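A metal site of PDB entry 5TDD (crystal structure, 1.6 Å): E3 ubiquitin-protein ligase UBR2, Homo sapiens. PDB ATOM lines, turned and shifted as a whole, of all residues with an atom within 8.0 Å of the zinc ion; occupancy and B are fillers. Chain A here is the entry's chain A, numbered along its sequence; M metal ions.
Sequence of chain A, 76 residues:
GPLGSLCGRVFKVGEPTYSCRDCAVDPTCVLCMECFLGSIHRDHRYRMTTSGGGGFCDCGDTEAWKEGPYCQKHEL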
ATOM      1  N   SER A  19      28.045  -3.893  -0.831  1.00  0.00           N
ATOM      2  CA  SER A  19      27.430  -5.148  -0.467  1.00  0.00           C
ATOM      3  C   SER A  19      28.300  -5.813   0.601  1.00  0.00           C
ATOM      4  O   SER A  19      29.435  -5.395   0.860  1.00  0.00           O
ATOM      5  CB  SER A  19      27.249  -6.063  -1.702  1.00  0.00           C
ATOM      6  OG  SER A  19      26.432  -7.185  -1.415  1.00  0.00           O
ATOM      7  N   CYS A  20      27.716  -6.766   1.283  1.00  0.00           N
ATOM      8  CA  CYS A  20      28.435  -7.555   2.273  1.00  0.00           C
ATOM      9  C   CYS A  20      28.492  -8.990   1.788  1.00  0.00           C
ATOM     10  O   CYS A  20      27.435  -9.616   1.617  1.00  0.00           O
ATOM     11  CB  CYS A  20      27.778  -7.502   3.637  1.00  0.00           C
ATOM     12  SG  CYS A  20      28.770  -8.387   4.846  1.00  0.00           S
ATOM     13  N   ARG A  21      29.698  -9.503   1.558  1.00  0.00           N
ATOM     14  CA  ARG A  21      29.840 -10.867   1.089  1.00  0.00           C
ATOM     15  C   ARG A  21      29.362 -11.866   2.122  1.00  0.00           C
ATOM     16  O   ARG A  21      29.001 -12.993   1.766  1.00  0.00           O
ATOM     17  CB  ARG A  21      31.282 -11.145   0.697  1.00  0.00           C
ATOM     18  CG  ARG A  21      31.663 -10.486  -0.654  1.00  0.00           C
ATOM     19  CD  ARG A  21      32.929 -11.095  -1.218  1.00  0.00           C
ATOM     20  NE  ARG A  21      33.993 -10.188  -0.913  1.00  0.00           N
ATOM     21  CZ  ARG A  21      34.530  -9.336  -1.782  1.00  0.00           C
ATOM     22  NH1 ARG A  21      34.127  -9.321  -3.053  1.00  0.00           N
ATOM     23  NH2 ARG A  21      35.474  -8.527  -1.367  1.00  0.00           N
ATOM     24  N   ASP A  22      29.398 -11.496   3.385  1.00  0.00           N
ATOM     25  CA  ASP A  22      28.964 -12.393   4.431  1.00  0.00           C
ATOM     26  C   ASP A  22      27.447 -12.398   4.595  1.00  0.00           C
ATOM     27  O   ASP A  22      26.865 -13.438   4.897  1.00  0.00           O
ATOM     28  CB  ASP A  22      29.628 -11.998   5.753  1.00  0.00           C
ATOM     29  CG  ASP A  22      31.127 -12.023   5.684  1.00  0.00           C
ATOM     30  OD1 ASP A  22      31.765 -11.108   6.203  1.00  0.00           O
ATOM     31  OD2 ASP A  22      31.664 -13.008   5.138  1.00  0.00           O
ATOM     32  N   CYS A  23      26.797 -11.243   4.416  1.00  0.00           N
ATOM     33  CA  CYS A  23      25.388 -11.148   4.793  1.00  0.00           C
ATOM     34  C   CYS A  23      24.423 -10.959   3.636  1.00  0.00           C
ATOM     35  O   CYS A  23      23.225 -11.182   3.825  1.00  0.00           O
ATOM     36  CB  CYS A  23      25.190  -9.965   5.757  1.00  0.00           C
ATOM     37  SG  CYS A  23      26.270 -10.100   7.263  1.00  0.00           S
ATOM     38  N   ALA A  24      24.880 -10.495   2.476  1.00  0.00           N
ATOM     39  CA  ALA A  24      23.937 -10.216   1.399  1.00  0.00           C
ATOM     40  C   ALA A  24      23.258 -11.499   0.925  1.00  0.00           C
ATOM     41  O   ALA A  24      23.925 -12.509   0.697  1.00  0.00           O
ATOM     42  CB  ALA A  24      24.677  -9.571   0.234  1.00  0.00           C
ATOM     43  N   LEU A  31      24.158  -1.214   0.063  1.00  0.00           N
ATOM     44  CA  LEU A  31      23.917  -0.084   0.947  1.00  0.00           C
ATOM     45  C   LEU A  31      24.628   1.156   0.414  1.00  0.00           C
ATOM     46  O   LEU A  31      25.709   1.068  -0.170  1.00  0.00           O
ATOM     47  CB  LEU A  31      24.442  -0.350   2.360  1.00  0.00           C
ATOM     48  CG  LEU A  31      23.937  -1.606   3.040  1.00  0.00           C
ATOM     49  CD1 LEU A  31      24.747  -1.869   4.302  1.00  0.00           C
ATOM     50  CD2 LEU A  31      22.448  -1.451   3.378  1.00  0.00           C
ATOM     51  N   PHE A  36      26.056   2.013   5.074  1.00  0.00           N
ATOM     52  CA  PHE A  36      27.174   1.099   5.260  1.00  0.00           C
ATOM     53  C   PHE A  36      27.988   1.470   6.492  1.00  0.00           C
ATOM     54  O   PHE A  36      28.279   0.609   7.341  1.00  0.00           O
ATOM     55  CB  PHE A  36      28.072   1.123   3.997  1.00  0.00           C
ATOM     56  CG  PHE A  36      29.366   0.400   4.169  1.00  0.00           C
ATOM     57  CD1 PHE A  36      29.400  -0.975   4.343  1.00  0.00           C
ATOM     58  CD2 PHE A  36      30.571   1.099   4.159  1.00  0.00           C
ATOM     59  CE1 PHE A  36      30.589  -1.633   4.519  1.00  0.00           C
ATOM     60  CE2 PHE A  36      31.748   0.449   4.315  1.00  0.00           C
ATOM     61  CZ  PHE A  36      31.761  -0.919   4.489  1.00  0.00           C
ATOM     62  N   SER A  39      26.443   0.570   9.780  1.00  0.00           N
ATOM     63  CA  SER A  39      25.970  -0.807   9.842  1.00  0.00           C
ATOM     64  C   SER A  39      27.049  -1.743  10.393  1.00  0.00           C
ATOM     65  O   SER A  39      28.242  -1.435  10.410  1.00  0.00           O
ATOM     66  CB  SER A  39      25.551  -1.298   8.466  1.00  0.00           C
ATOM     67  OG  SER A  39      26.652  -1.709   7.681  1.00  0.00           O
ATOM     68  N   ILE A  40      26.603  -2.933  10.792  1.00  0.00           N
ATOM     69  CA  ILE A  40      27.541  -3.950  11.251  1.00  0.00           C
ATOM     70  C   ILE A  40      28.483  -4.392  10.133  1.00  0.00           C
ATOM     71  O   ILE A  40      29.552  -4.951  10.400  1.00  0.00           O
ATOM     72  CB  ILE A  40      26.714  -5.132  11.827  1.00  0.00           C
ATOM     73  CG1 ILE A  40      27.567  -6.007  12.733  1.00  0.00           C
ATOM     74  CG2 ILE A  40      26.067  -5.956  10.726  1.00  0.00           C
ATOM     75  CD1 ILE A  40      27.719  -5.410  14.100  1.00  0.00           C
ATOM     76  N   HIS A  41      28.091  -4.191   8.872  1.00  0.00           N
ATOM     77  CA  HIS A  41      28.854  -4.719   7.754  1.00  0.00           C
ATOM     78  C   HIS A  41      30.149  -3.963   7.506  1.00  0.00           C
ATOM     79  O   HIS A  41      30.994  -4.463   6.765  1.00  0.00           O
ATOM     80  CB  HIS A  41      27.989  -4.744   6.469  1.00  0.00           C
ATOM     81  CG  HIS A  41      26.648  -5.326   6.716  1.00  0.00           C
ATOM     82  ND1 HIS A  41      26.480  -6.665   7.001  1.00  0.00           N
ATOM     83  CD2 HIS A  41      25.413  -4.755   6.836  1.00  0.00           C
ATOM     84  CE1 HIS A  41      25.199  -6.901   7.240  1.00  0.00           C
ATOM     85  NE2 HIS A  41      24.540  -5.762   7.140  1.00  0.00           N
ATOM     86  N   ARG A  42      30.327  -2.792   8.129  1.00  0.00           N
ATOM     87  CA  ARG A  42      31.602  -2.089   7.998  1.00  0.00           C
ATOM     88  C   ARG A  42      32.745  -2.895   8.586  1.00  0.00           C
ATOM     89  O   ARG A  42      33.912  -2.655   8.216  1.00  0.00           O
ATOM     90  CB  ARG A  42      31.520  -0.693   8.638  1.00  0.00           C
ATOM     91  CG  ARG A  42      31.474  -0.654  10.140  1.00  0.00           C
ATOM     92  CD  ARG A  42      31.366   0.798  10.637  1.00  0.00           C
ATOM     93  NE  ARG A  42      32.615   1.554  10.426  1.00  0.00           N
ATOM     94  CZ  ARG A  42      32.744   2.879  10.521  1.00  0.00           C
ATOM     95  NH1 ARG A  42      31.689   3.641  10.802  1.00  0.00           N
ATOM     96  NH2 ARG A  42      33.910   3.443  10.313  1.00  0.00           N
ATOM     97  N   ASP A  43      32.443  -3.877   9.428  1.00  0.00           N
ATOM     98  CA  ASP A  43      33.441  -4.764  10.022  1.00  0.00           C
ATOM     99  C   ASP A  43      33.470  -6.131   9.345  1.00  0.00           C
ATOM    100  O   ASP A  43      34.090  -7.060   9.879  1.00  0.00           O
ATOM    101  CB  ASP A  43      33.178  -4.950  11.508  1.00  0.00           C
ATOM    102  CG  ASP A  43      33.222  -3.655  12.295  1.00  0.00           C
ATOM    103  OD1 ASP A  43      34.161  -2.854  12.133  1.00  0.00           O
ATOM    104  OD2 ASP A  43      32.296  -3.470  13.119  1.00  0.00           O
ATOM    105  N   HIS A  44      32.793  -6.295   8.209  1.00  0.00           N
ATOM    106  CA  HIS A  44      32.662  -7.575   7.516  1.00  0.00           C
ATOM    107  C   HIS A  44      33.437  -7.532   6.203  1.00  0.00           C
ATOM    108  O   HIS A  44      34.106  -6.543   5.880  1.00  0.00           O
ATOM    109  CB  HIS A  44      31.188  -7.892   7.258  1.00  0.00           C
ATOM    110  CG  HIS A  44      30.380  -8.154   8.491  1.00  0.00           C
ATOM    111  ND1 HIS A  44      29.006  -8.325   8.465  1.00  0.00           N
ATOM    112  CD2 HIS A  44      30.748  -8.316   9.787  1.00  0.00           C
ATOM    113  CE1 HIS A  44      28.577  -8.542   9.693  1.00  0.00           C
ATOM    114  NE2 HIS A  44      29.616  -8.543  10.512  1.00  0.00           N
ATOM    115  N   ARG A  45      33.313  -8.602   5.421  1.00  0.00           N
ATOM    116  CA  ARG A  45      33.972  -8.684   4.111  1.00  0.00           C
ATOM    117  C   ARG A  45      33.105  -7.955   3.091  1.00  0.00           C
ATOM    118  O   ARG A  45      32.288  -8.549   2.387  1.00  0.00           O
ATOM    119  CB  ARG A  45      34.199 -10.135   3.693  1.00  0.00           C
ATOM    120  CG  ARG A  45      35.119 -10.907   4.593  1.00  0.00           C
ATOM    121  CD  ARG A  45      35.131 -12.384   4.195  1.00  0.00           C
ATOM    122  NE  ARG A  45      35.859 -13.159   5.170  1.00  0.00           N
ATOM    123  CZ  ARG A  45      35.307 -13.881   6.152  1.00  0.00           C
ATOM    124  NH1 ARG A  45      33.988 -13.943   6.315  1.00  0.00           N
ATOM    125  NH2 ARG A  45      36.097 -14.544   6.962  1.00  0.00           N
ATOM    126  N   TYR A  46      33.282  -6.660   2.996  1.00  0.00           N
ATOM    127  CA  TYR A  46      32.416  -5.866   2.121  1.00  0.00           C
ATOM    128  C   TYR A  46      32.983  -5.806   0.695  1.00  0.00           C
ATOM    129  O   TYR A  46      34.175  -6.048   0.451  1.00  0.00           O
ATOM    130  CB  TYR A  46      32.209  -4.480   2.742  1.00  0.00           C
ATOM    131  CG  TYR A  46      33.437  -3.618   2.821  1.00  0.00           C
ATOM    132  CD1 TYR A  46      34.151  -3.516   4.000  1.00  0.00           C
ATOM    133  CD2 TYR A  46      33.866  -2.862   1.729  1.00  0.00           C
ATOM    134  CE1 TYR A  46      35.278  -2.705   4.090  1.00  0.00           C
ATOM    135  CE2 TYR A  46      34.993  -2.052   1.819  1.00  0.00           C
ATOM    136  CZ  TYR A  46      35.699  -1.999   2.989  1.00  0.00           C
ATOM    137  OH  TYR A  46      36.820  -1.191   3.066  1.00  0.00           O
ATOM    138  N   TRP A  65      19.141  -9.254   3.686  1.00  0.00           N
ATOM    139  CA  TRP A  65      20.316  -9.377   4.548  1.00  0.00           C
ATOM    140  C   TRP A  65      20.125 -10.543   5.514  1.00  0.00           C
ATOM    141  O   TRP A  65      19.088 -10.636   6.172  1.00  0.00           O
ATOM    142  CB  TRP A  65      20.566  -8.070   5.330  1.00  0.00           C
ATOM    143  CG  TRP A  65      20.680  -6.897   4.422  1.00  0.00           C
ATOM    144  CD1 TRP A  65      19.712  -5.997   4.162  1.00  0.00           C
ATOM    145  CD2 TRP A  65      21.803  -6.537   3.609  1.00  0.00           C
ATOM    146  NE1 TRP A  65      20.168  -5.046   3.269  1.00  0.00           N
ATOM    147  CE2 TRP A  65      21.441  -5.376   2.903  1.00  0.00           C
ATOM    148  CE3 TRP A  65      23.081  -7.064   3.436  1.00  0.00           C
ATOM    149  CZ2 TRP A  65      22.299  -4.748   2.037  1.00  0.00           C
ATOM    150  CZ3 TRP A  65      23.918  -6.455   2.559  1.00  0.00           C
ATOM    151  CH2 TRP A  65      23.532  -5.294   1.872  1.00  0.00           C
ATOM    152  N   LYS A  66      21.132 -11.414   5.607  1.00  0.00           N
ATOM    153  CA  LYS A  66      21.044 -12.538   6.547  1.00  0.00           C
ATOM    154  C   LYS A  66      21.149 -12.060   8.002  1.00  0.00           C
ATOM    155  O   LYS A  66      20.648 -12.737   8.911  1.00  0.00           O
ATOM    156  CB  LYS A  66      22.145 -13.544   6.251  1.00  0.00           C
ATOM    157  CG  LYS A  66      22.098 -14.079   4.846  1.00  0.00           C
ATOM    158  CD  LYS A  66      23.323 -14.937   4.546  1.00  0.00           C
ATOM    159  CE  LYS A  66      23.460 -15.199   3.074  1.00  0.00           C
ATOM    160  NZ  LYS A  66      24.720 -15.956   2.808  1.00  0.00           N
ATOM    161  N   GLU A  67      21.827 -10.948   8.236  1.00  0.00           N
ATOM    162  CA  GLU A  67      21.797 -10.271   9.527  1.00  0.00           C
ATOM    163  C   GLU A  67      22.124  -8.813   9.254  1.00  0.00           C
ATOM    164  O   GLU A  67      22.578  -8.459   8.158  1.00  0.00           O
ATOM    165  CB  GLU A  67      22.759 -10.869  10.545  1.00  0.00           C
ATOM    166  CG  GLU A  67      24.213 -10.719  10.204  1.00  0.00           C
ATOM    167  CD  GLU A  67      25.141 -11.335  11.265  1.00  0.00           C
ATOM    168  OE1 GLU A  67      24.932 -12.518  11.638  1.00  0.00           O
ATOM    169  OE2 GLU A  67      26.065 -10.646  11.716  1.00  0.00           O
ATOM    170  N   GLY A  68      21.797  -7.958  10.215  1.00  0.00           N
ATOM    171  CA  GLY A  68      22.056  -6.545  10.110  1.00  0.00           C
ATOM    172  C   GLY A  68      21.344  -5.867   8.958  1.00  0.00           C
ATOM    173  O   GLY A  68      21.970  -5.173   8.145  1.00  0.00           O
HETATM  174 ZN    ZN M   1      27.697  -8.320   6.872  1.00  0.00          ZN
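The backbone NH (N) of His 41 lies close to the side-chain hydroxyl (OG) of Ser 39. The backbone carbonyl oxygen (O) of Glu 67 lies close to a ring nitrogen (NE2) of His 41, 3.5 Å away. The backbone carbonyl oxygen (O) of Gly 68 sits at hydrogen-bond distance from a ring nitrogen (NE2) of His 41. The side-chain sulfur of Cys 20 lies close to the backbone NH of Asp 22 (3.5 Å). The backbone NH (N) of Lys 66 lies within hydrogen-bond range of the backbone carbonyl oxygen (O) of Cys 23 (2.8 Å).
The zinc ion is bound by ND1 of His 41 (2.1 Å), ND1 of His 44 (2.1 Å), SG of Cys 20 (2.3 Å) and SG of Cys 23 (2.3 Å).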
